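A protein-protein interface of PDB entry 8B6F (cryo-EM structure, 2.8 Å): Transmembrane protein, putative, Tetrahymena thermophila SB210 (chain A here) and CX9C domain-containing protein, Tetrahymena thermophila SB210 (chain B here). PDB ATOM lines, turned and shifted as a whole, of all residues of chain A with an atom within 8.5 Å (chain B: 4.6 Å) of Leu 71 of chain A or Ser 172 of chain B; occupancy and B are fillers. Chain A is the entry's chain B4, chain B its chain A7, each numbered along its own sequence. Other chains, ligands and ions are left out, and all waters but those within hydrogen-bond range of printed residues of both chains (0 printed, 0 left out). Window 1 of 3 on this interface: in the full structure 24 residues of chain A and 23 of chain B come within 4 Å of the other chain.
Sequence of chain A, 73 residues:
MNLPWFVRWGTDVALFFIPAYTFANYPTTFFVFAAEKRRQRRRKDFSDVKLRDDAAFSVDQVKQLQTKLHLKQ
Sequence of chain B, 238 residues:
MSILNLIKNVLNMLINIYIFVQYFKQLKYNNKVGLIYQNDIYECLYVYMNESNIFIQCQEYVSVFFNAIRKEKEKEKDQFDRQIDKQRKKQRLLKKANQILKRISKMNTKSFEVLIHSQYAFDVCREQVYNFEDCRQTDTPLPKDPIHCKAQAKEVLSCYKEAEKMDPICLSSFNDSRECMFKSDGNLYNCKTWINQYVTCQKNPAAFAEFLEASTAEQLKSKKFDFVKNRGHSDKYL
Of the 16 printed residues of chain A, 9 touch a printed residue of chain B. Printed residues of chain A that touch a printed residue of chain B: Arg 43, Lys 44, Phe 46, Val 49, Val 62, Leu 69, His 70, Leu 71 and Gln 73. Hydrophobic or aromatic side chains of chain B within 4 Å of the printed part of chain A: Ile 169, Leu 171 and Leu 220. Among the printed residues, 12 pairs touch across the chains. Among the printed residues, no Asp or Glu carboxylate lies within 4 Å of a Lys or Arg side-chain nitrogen of the other chain.
The backbone carbonyl oxygen (O) of Leu 71 of chain A is in hydrogen-bond range of the backbone NH (N) of Lys 221 of chain B, at 3.3 Å. O of Leu 220 of chain B sits close to O of Leu 71 of chain A (3.4 Å). The backbone NH of Lys 44 of chain A lies within hydrogen-bond range of the side-chain amide oxygen of Asn 175 of chain B, 3.2 Å away.
O of Leu 171 of chain B is in hydrogen-bond range of ND2 of Asn 175 of chain B, 3.2 Å away. N of Leu 71 of chain A lies within hydrogen-bond range of O of Gln 66 of chain A (3.3 Å). A ring nitrogen (ND1) of His 70 of chain A is in hydrogen-bond range of the backbone carbonyl oxygen (O) of Lys 68 of chain A, at 2.9 Å.
Of the printed residues of chain B, Lys 44 of chain A touches Asn 175 (3.2 Å). Of the printed residues of chain B, Val 49 of chain A touches Leu 171. Printed residues of chain B within 4 Å of Leu 69 of chain A: Leu 220. Of chain B, only Ser 172, Leu 220 and Lys 221 come within 4 Å of Leu 71 of chain A. Printed residues of chain B within 4 Å of Gln 73 of chain A: Lys 221 (3.6 Å). Of the printed residues of chain A, Ser 172 of chain B touches Arg 43 (3.9 Å) and Leu 71 (3.97 Å). No residue of chain A comes within 4 Å of Ser 173 of chain B. Printed residues of chain A within 4 Å of Leu 220 of chain B: Leu 69, His 70 and Leu 71. The nearest printed residue of chain B that does not touch Leu 71 of chain A is Ser 173 of chain B (6.7 Å). The nearest residue of chain A that does not touch Ser 172 of chain B is Gln 66 of chain A (4.1 Å).
NH1 of Arg 43 of chain A touches O of Ser 172 of chain B, at 3.9 Å. Asn 175 of chain B touches Arg 43 of chain A (CB to NH1, 3.1 Å). Phe 46 of chain A touches Leu 171 of chain B. CG1 of Val 49 of chain A touches CD1 of Leu 171 of chain B, 3.8 Å away. CG2 of Val 62 of chain A touches N of Ile 169 of chain B (3.4 Å). Leu 220 of chain B touches Leu 69 of chain A (CD1 to O, 3.3 Å). Leu 220 of chain B touches His 70 of chain A (CB to O, 3.6 Å). Ser 172 of chain B touches Leu 71 of chain A (OG to CD1, 3.97 Å). OE1 of Gln 73 of chain A touches NZ of Lys 221 of chain B, at 3.6 Å.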
ATOM      1  N   ARG A  43      10.822 -13.647 -19.253  1.00  0.00           N
ATOM      2  CA  ARG A  43       9.702 -13.437 -18.347  1.00  0.00           C
ATOM      3  C   ARG A  43      10.210 -13.055 -16.963  1.00  0.00           C
ATOM      4  O   ARG A  43      11.096 -13.710 -16.409  1.00  0.00           O
ATOM      5  CB  ARG A  43       8.849 -14.705 -18.276  1.00  0.00           C
ATOM      6  CG  ARG A  43       7.632 -14.586 -17.376  1.00  0.00           C
ATOM      7  CD  ARG A  43       6.686 -15.756 -17.576  1.00  0.00           C
ATOM      8  NE  ARG A  43       6.062 -15.728 -18.894  1.00  0.00           N
ATOM      9  CZ  ARG A  43       4.907 -15.139 -19.172  1.00  0.00           C
ATOM     10  NH1 ARG A  43       4.201 -14.521 -18.239  1.00  0.00           N
ATOM     11  NH2 ARG A  43       4.446 -15.173 -20.419  1.00  0.00           N
ATOM     12  N   LYS A  44       9.642 -11.986 -16.408  1.00  0.00           N
ATOM     13  CA  LYS A  44      10.131 -11.423 -15.160  1.00  0.00           C
ATOM     14  C   LYS A  44       9.606 -12.214 -13.963  1.00  0.00           C
ATOM     15  O   LYS A  44       8.775 -13.118 -14.090  1.00  0.00           O
ATOM     16  CB  LYS A  44       9.729  -9.954 -15.039  1.00  0.00           C
ATOM     17  CG  LYS A  44      10.791  -8.980 -15.523  1.00  0.00           C
ATOM     18  CD  LYS A  44      10.364  -7.542 -15.281  1.00  0.00           C
ATOM     19  CE  LYS A  44      11.434  -6.558 -15.722  1.00  0.00           C
ATOM     20  NZ  LYS A  44      12.689  -6.695 -14.936  1.00  0.00           N
ATOM     21  N   PHE A  46       8.795 -11.987  -9.397  1.00  0.00           N
ATOM     22  CA  PHE A  46       8.374 -11.102  -8.315  1.00  0.00           C
ATOM     23  C   PHE A  46       9.555 -10.335  -7.736  1.00  0.00           C
ATOM     24  O   PHE A  46       9.457  -9.132  -7.474  1.00  0.00           O
ATOM     25  CB  PHE A  46       7.673 -11.907  -7.222  1.00  0.00           C
ATOM     26  CG  PHE A  46       6.473 -12.666  -7.706  1.00  0.00           C
ATOM     27  CD1 PHE A  46       5.249 -12.033  -7.846  1.00  0.00           C
ATOM     28  CD2 PHE A  46       6.563 -14.013  -8.010  1.00  0.00           C
ATOM     29  CE1 PHE A  46       4.140 -12.727  -8.289  1.00  0.00           C
ATOM     30  CE2 PHE A  46       5.458 -14.713  -8.453  1.00  0.00           C
ATOM     31  CZ  PHE A  46       4.244 -14.069  -8.592  1.00  0.00           C
ATOM     32  N   VAL A  49      10.589  -7.550 -10.169  1.00  0.00           N
ATOM     33  CA  VAL A  49       9.678  -6.412 -10.114  1.00  0.00           C
ATOM     34  C   VAL A  49       9.557  -5.920  -8.675  1.00  0.00           C
ATOM     35  O   VAL A  49       9.927  -6.605  -7.719  1.00  0.00           O
ATOM     36  CB  VAL A  49       8.298  -6.772 -10.698  1.00  0.00           C
ATOM     37  CG1 VAL A  49       8.436  -7.296 -12.119  1.00  0.00           C
ATOM     38  CG2 VAL A  49       7.585  -7.788  -9.815  1.00  0.00           C
ATOM     39  N   VAL A  62      -0.806 -15.802  -4.846  1.00  0.00           N
ATOM     40  CA  VAL A  62      -0.832 -15.723  -6.304  1.00  0.00           C
ATOM     41  C   VAL A  62      -0.282 -17.007  -6.911  1.00  0.00           C
ATOM     42  O   VAL A  62      -0.834 -17.540  -7.880  1.00  0.00           O
ATOM     43  CB  VAL A  62      -0.056 -14.484  -6.788  1.00  0.00           C
ATOM     44  CG1 VAL A  62       0.135 -14.514  -8.301  1.00  0.00           C
ATOM     45  CG2 VAL A  62      -0.781 -13.216  -6.375  1.00  0.00           C
ATOM     46  N   LYS A  63       0.815 -17.525  -6.355  1.00  0.00           N
ATOM     47  CA  LYS A  63       1.381 -18.769  -6.868  1.00  0.00           C
ATOM     48  C   LYS A  63       0.401 -19.923  -6.709  1.00  0.00           C
ATOM     49  O   LYS A  63       0.243 -20.743  -7.620  1.00  0.00           O
ATOM     50  CB  LYS A  63       2.697 -19.080  -6.157  1.00  0.00           C
ATOM     51  CG  LYS A  63       3.837 -18.147  -6.531  1.00  0.00           C
ATOM     52  CD  LYS A  63       5.120 -18.531  -5.812  1.00  0.00           C
ATOM     53  CE  LYS A  63       6.271 -17.621  -6.209  1.00  0.00           C
ATOM     54  NZ  LYS A  63       7.531 -17.972  -5.494  1.00  0.00           N
ATOM     55  N   GLN A  64      -0.265 -20.009  -5.556  1.00  0.00           N
ATOM     56  CA  GLN A  64      -1.244 -21.071  -5.351  1.00  0.00           C
ATOM     57  C   GLN A  64      -2.406 -20.942  -6.326  1.00  0.00           C
ATOM     58  O   GLN A  64      -2.886 -21.945  -6.868  1.00  0.00           O
ATOM     59  CB  GLN A  64      -1.751 -21.048  -3.909  1.00  0.00           C
ATOM     60  CG  GLN A  64      -0.705 -21.444  -2.877  1.00  0.00           C
ATOM     61  CD  GLN A  64      -0.138 -22.833  -3.111  1.00  0.00           C
ATOM     62  OE1 GLN A  64       1.054 -23.067  -2.913  1.00  0.00           O
ATOM     63  NE2 GLN A  64      -0.988 -23.764  -3.531  1.00  0.00           N
ATOM     64  N   LEU A  65      -2.876 -19.717  -6.559  1.00  0.00           N
ATOM     65  CA  LEU A  65      -3.963 -19.516  -7.513  1.00  0.00           C
ATOM     66  C   LEU A  65      -3.544 -19.933  -8.917  1.00  0.00           C
ATOM     67  O   LEU A  65      -4.306 -20.595  -9.630  1.00  0.00           O
ATOM     68  CB  LEU A  65      -4.403 -18.051  -7.498  1.00  0.00           C
ATOM     69  CG  LEU A  65      -5.573 -17.689  -8.415  1.00  0.00           C
ATOM     70  CD1 LEU A  65      -6.854 -18.357  -7.943  1.00  0.00           C
ATOM     71  CD2 LEU A  65      -5.747 -16.182  -8.489  1.00  0.00           C
ATOM     72  N   GLN A  66      -2.332 -19.559  -9.330  1.00  0.00           N
ATOM     73  CA  GLN A  66      -1.853 -19.944 -10.654  1.00  0.00           C
ATOM     74  C   GLN A  66      -1.723 -21.458 -10.772  1.00  0.00           C
ATOM     75  O   GLN A  66      -2.073 -22.040 -11.805  1.00  0.00           O
ATOM     76  CB  GLN A  66      -0.516 -19.263 -10.947  1.00  0.00           C
ATOM     77  CG  GLN A  66      -0.630 -17.758 -11.134  1.00  0.00           C
ATOM     78  CD  GLN A  66       0.703 -17.110 -11.438  1.00  0.00           C
ATOM     79  OE1 GLN A  66       1.736 -17.776 -11.475  1.00  0.00           O
ATOM     80  NE2 GLN A  66       0.687 -15.799 -11.661  1.00  0.00           N
ATOM     81  N   THR A  67      -1.218 -22.113  -9.725  1.00  0.00           N
ATOM     82  CA  THR A  67      -1.118 -23.568  -9.747  1.00  0.00           C
ATOM     83  C   THR A  67      -2.495 -24.210  -9.854  1.00  0.00           C
ATOM     84  O   THR A  67      -2.680 -25.179 -10.600  1.00  0.00           O
ATOM     85  CB  THR A  67      -0.394 -24.063  -8.493  1.00  0.00           C
ATOM     86  OG1 THR A  67       0.967 -23.614  -8.512  1.00  0.00           O
ATOM     87  CG2 THR A  67      -0.416 -25.589  -8.409  1.00  0.00           C
ATOM     88  N   LYS A  68      -3.473 -23.690  -9.111  1.00  0.00           N
ATOM     89  CA  LYS A  68      -4.818 -24.254  -9.163  1.00  0.00           C
ATOM     90  C   LYS A  68      -5.442 -24.075 -10.541  1.00  0.00           C
ATOM     91  O   LYS A  68      -6.087 -24.992 -11.061  1.00  0.00           O
ATOM     92  CB  LYS A  68      -5.693 -23.606  -8.090  1.00  0.00           C
ATOM     93  CG  LYS A  68      -7.100 -24.180  -8.015  1.00  0.00           C
ATOM     94  CD  LYS A  68      -7.866 -23.633  -6.820  1.00  0.00           C
ATOM     95  CE  LYS A  68      -8.210 -22.161  -6.986  1.00  0.00           C
ATOM     96  NZ  LYS A  68      -9.141 -21.930  -8.124  1.00  0.00           N
ATOM     97  N   LEU A  69      -5.269 -22.901 -11.146  1.00  0.00           N
ATOM     98  CA  LEU A  69      -5.876 -22.621 -12.440  1.00  0.00           C
ATOM     99  C   LEU A  69      -5.096 -23.204 -13.610  1.00  0.00           C
ATOM    100  O   LEU A  69      -5.631 -23.250 -14.722  1.00  0.00           O
ATOM    101  CB  LEU A  69      -6.018 -21.110 -12.639  1.00  0.00           C
ATOM    102  CG  LEU A  69      -7.293 -20.472 -12.082  1.00  0.00           C
ATOM    103  CD1 LEU A  69      -7.420 -20.720 -10.589  1.00  0.00           C
ATOM    104  CD2 LEU A  69      -7.315 -18.982 -12.381  1.00  0.00           C
ATOM    105  N   HIS A  70      -3.861 -23.654 -13.394  1.00  0.00           N
ATOM    106  CA  HIS A  70      -3.015 -24.138 -14.482  1.00  0.00           C
ATOM    107  C   HIS A  70      -2.847 -23.051 -15.543  1.00  0.00           C
ATOM    108  O   HIS A  70      -3.121 -23.254 -16.727  1.00  0.00           O
ATOM    109  CB  HIS A  70      -3.589 -25.417 -15.096  1.00  0.00           C
ATOM    110  CG  HIS A  70      -3.993 -26.443 -14.085  1.00  0.00           C
ATOM    111  ND1 HIS A  70      -5.224 -26.428 -13.461  1.00  0.00           N
ATOM    112  CD2 HIS A  70      -3.333 -27.513 -13.586  1.00  0.00           C
ATOM    113  CE1 HIS A  70      -5.302 -27.445 -12.623  1.00  0.00           C
ATOM    114  NE2 HIS A  70      -4.168 -28.120 -12.679  1.00  0.00           N
ATOM    115  N   LEU A  71      -2.391 -21.878 -15.101  1.00  0.00           N
ATOM    116  CA  LEU A  71      -2.357 -20.714 -15.980  1.00  0.00           C
ATOM    117  C   LEU A  71      -1.452 -20.958 -17.183  1.00  0.00           C
ATOM    118  O   LEU A  71      -1.831 -20.675 -18.325  1.00  0.00           O
ATOM    119  CB  LEU A  71      -1.897 -19.486 -15.193  1.00  0.00           C
ATOM    120  CG  LEU A  71      -2.300 -18.105 -15.728  1.00  0.00           C
ATOM    121  CD1 LEU A  71      -1.912 -17.025 -14.736  1.00  0.00           C
ATOM    122  CD2 LEU A  71      -1.696 -17.802 -17.093  1.00  0.00           C
ATOM    123  N   LYS A  72      -0.265 -21.507 -16.953  1.00  0.00           N
ATOM    124  CA  LYS A  72       0.703 -21.754 -18.015  1.00  0.00           C
ATOM    125  C   LYS A  72       0.854 -23.252 -18.231  1.00  0.00           C
ATOM    126  O   LYS A  72       1.135 -23.998 -17.285  1.00  0.00           O
ATOM    127  CB  LYS A  72       2.057 -21.128 -17.678  1.00  0.00           C
ATOM    128  CG  LYS A  72       2.086 -19.611 -17.824  1.00  0.00           C
ATOM    129  CD  LYS A  72       3.496 -19.055 -17.659  1.00  0.00           C
ATOM    130  CE  LYS A  72       3.969 -19.118 -16.213  1.00  0.00           C
ATOM    131  NZ  LYS A  72       3.170 -18.237 -15.313  1.00  0.00           N
ATOM    132  N   GLN A  73       0.667 -23.685 -19.473  1.00  0.00           N
ATOM    133  CA  GLN A  73       0.822 -25.087 -19.837  1.00  0.00           C
ATOM    134  C   GLN A  73       1.316 -25.213 -21.273  1.00  0.00           C
ATOM    135  O   GLN A  73       1.788 -26.271 -21.688  1.00  0.00           O
ATOM    136  CB  GLN A  73      -0.500 -25.837 -19.669  1.00  0.00           C
ATOM    137  CG  GLN A  73      -0.892 -26.079 -18.220  1.00  0.00           C
ATOM    138  CD  GLN A  73      -2.116 -26.960 -18.090  1.00  0.00           C
ATOM    139  OE1 GLN A  73      -3.039 -26.884 -18.901  1.00  0.00           O
ATOM    140  NE2 GLN A  73      -2.127 -27.810 -17.070  1.00  0.00           N
ATOM    141  OXT GLN A  73       1.256 -24.261 -22.051  1.00  0.00           O
ATOM    142  N   ILE B 169      -0.341 -10.458  -8.306  1.00  0.00           N
ATOM    143  CA  ILE B 169      -1.310 -11.070  -9.205  1.00  0.00           C
ATOM    144  C   ILE B 169      -1.243 -10.452 -10.592  1.00  0.00           C
ATOM    145  O   ILE B 169      -1.652 -11.083 -11.573  1.00  0.00           O
ATOM    146  CB  ILE B 169      -2.729 -10.949  -8.606  1.00  0.00           C
ATOM    147  CG1 ILE B 169      -3.710 -11.828  -9.388  1.00  0.00           C
ATOM    148  CG2 ILE B 169      -3.187  -9.492  -8.601  1.00  0.00           C
ATOM    149  CD1 ILE B 169      -5.099 -11.887  -8.786  1.00  0.00           C
ATOM    150  N   CYS B 170      -0.737  -9.225 -10.700  1.00  0.00           N
ATOM    151  CA  CYS B 170      -0.586  -8.556 -11.984  1.00  0.00           C
ATOM    152  C   CYS B 170       0.644  -9.011 -12.754  1.00  0.00           C
ATOM    153  O   CYS B 170       0.823  -8.590 -13.902  1.00  0.00           O
ATOM    154  CB  CYS B 170      -0.499  -7.044 -11.778  1.00  0.00           C
ATOM    155  SG  CYS B 170      -2.065  -6.198 -11.522  1.00  0.00           S
ATOM    156  N   LEU B 171       1.491  -9.853 -12.161  1.00  0.00           N
ATOM    157  CA  LEU B 171       2.775 -10.161 -12.779  1.00  0.00           C
ATOM    158  C   LEU B 171       2.597 -10.897 -14.101  1.00  0.00           C
ATOM    159  O   LEU B 171       3.299 -10.611 -15.078  1.00  0.00           O
ATOM    160  CB  LEU B 171       3.634 -10.983 -11.819  1.00  0.00           C
ATOM    161  CG  LEU B 171       5.053 -11.296 -12.300  1.00  0.00           C
ATOM    162  CD1 LEU B 171       5.835 -10.021 -12.569  1.00  0.00           C
ATOM    163  CD2 LEU B 171       5.779 -12.160 -11.291  1.00  0.00           C
ATOM    164  N   SER B 172       1.661 -11.846 -14.158  1.00  0.00           N
ATOM    165  CA  SER B 172       1.455 -12.596 -15.393  1.00  0.00           C
ATOM    166  C   SER B 172       0.990 -11.681 -16.518  1.00  0.00           C
ATOM    167  O   SER B 172       1.482 -11.776 -17.647  1.00  0.00           O
ATOM    168  CB  SER B 172       0.449 -13.725 -15.164  1.00  0.00           C
ATOM    169  OG  SER B 172      -0.792 -13.220 -14.699  1.00  0.00           O
ATOM    170  N   SER B 173       0.039 -10.791 -16.231  1.00  0.00           N
ATOM    171  CA  SER B 173      -0.421  -9.858 -17.253  1.00  0.00           C
ATOM    172  C   SER B 173       0.706  -8.933 -17.692  1.00  0.00           C
ATOM    173  O   SER B 173       0.850  -8.638 -18.882  1.00  0.00           O
ATOM    174  CB  SER B 173      -1.604  -9.044 -16.730  1.00  0.00           C
ATOM    175  OG  SER B 173      -2.662  -9.894 -16.325  1.00  0.00           O
ATOM    176  N   PHE B 174       1.502  -8.444 -16.740  1.00  0.00           N
ATOM    177  CA  PHE B 174       2.617  -7.574 -17.093  1.00  0.00           C
ATOM    178  C   PHE B 174       3.624  -8.306 -17.970  1.00  0.00           C
ATOM    179  O   PHE B 174       4.141  -7.742 -18.941  1.00  0.00           O
ATOM    180  CB  PHE B 174       3.287  -7.045 -15.825  1.00  0.00           C
ATOM    181  CG  PHE B 174       4.295  -5.960 -16.079  1.00  0.00           C
ATOM    182  CD1 PHE B 174       3.920  -4.778 -16.697  1.00  0.00           C
ATOM    183  CD2 PHE B 174       5.613  -6.113 -15.683  1.00  0.00           C
ATOM    184  CE1 PHE B 174       4.841  -3.775 -16.925  1.00  0.00           C
ATOM    185  CE2 PHE B 174       6.538  -5.114 -15.908  1.00  0.00           C
ATOM    186  CZ  PHE B 174       6.152  -3.943 -16.530  1.00  0.00           C
ATOM    187  N   ASN B 175       3.908  -9.572 -17.651  1.00  0.00           N
ATOM    188  CA  ASN B 175       4.869 -10.336 -18.439  1.00  0.00           C
ATOM    189  C   ASN B 175       4.367 -10.592 -19.854  1.00  0.00           C
ATOM    190  O   ASN B 175       5.133 -10.478 -20.817  1.00  0.00           O
ATOM    191  CB  ASN B 175       5.179 -11.658 -17.743  1.00  0.00           C
ATOM    192  CG  ASN B 175       6.040 -11.480 -16.515  1.00  0.00           C
ATOM    193  OD1 ASN B 175       6.827 -10.539 -16.430  1.00  0.00           O
ATOM    194  ND2 ASN B 175       5.899 -12.385 -15.555  1.00  0.00           N
ATOM    195  N   ASP B 176       3.088 -10.940 -20.011  1.00  0.00           N
ATOM    196  CA  ASP B 176       2.574 -11.183 -21.354  1.00  0.00           C
ATOM    197  C   ASP B 176       2.543  -9.894 -22.163  1.00  0.00           C
ATOM    198  O   ASP B 176       2.806  -9.904 -23.371  1.00  0.00           O
ATOM    199  CB  ASP B 176       1.193 -11.847 -21.291  1.00  0.00           C
ATOM    200  CG  ASP B 176       0.101 -10.919 -20.786  1.00  0.00           C
ATOM    201  OD1 ASP B 176       0.184  -9.692 -20.993  1.00  0.00           O
ATOM    202  OD2 ASP B 176      -0.865 -11.433 -20.182  1.00  0.00           O
ATOM    203  N   LEU B 220      -5.988 -20.243 -20.681  1.00  0.00           N
ATOM    204  CA  LEU B 220      -5.009 -20.784 -19.738  1.00  0.00           C
ATOM    205  C   LEU B 220      -3.914 -21.543 -20.492  1.00  0.00           C
ATOM    206  O   LEU B 220      -3.700 -22.741 -20.309  1.00  0.00           O
ATOM    207  CB  LEU B 220      -5.701 -21.683 -18.724  1.00  0.00           C
ATOM    208  CG  LEU B 220      -6.774 -21.023 -17.857  1.00  0.00           C
ATOM    209  CD1 LEU B 220      -7.594 -22.080 -17.137  1.00  0.00           C
ATOM    210  CD2 LEU B 220      -6.150 -20.059 -16.863  1.00  0.00           C
ATOM    211  N   LYS B 221      -3.211 -20.814 -21.356  1.00  0.00           N
ATOM    212  CA  LYS B 221      -2.157 -21.400 -22.169  1.00  0.00           C
ATOM    213  C   LYS B 221      -1.045 -20.382 -22.359  1.00  0.00           C
ATOM    214  O   LYS B 221      -1.243 -19.175 -22.198  1.00  0.00           O
ATOM    215  CB  LYS B 221      -2.680 -21.866 -23.535  1.00  0.00           C
ATOM    216  CG  LYS B 221      -3.632 -23.053 -23.476  1.00  0.00           C
ATOM    217  CD  LYS B 221      -2.924 -24.317 -23.001  1.00  0.00           C
ATOM    218  CE  LYS B 221      -3.872 -25.507 -22.984  1.00  0.00           C
ATOM    219  NZ  LYS B 221      -3.196 -26.753 -22.526  1.00  0.00           N
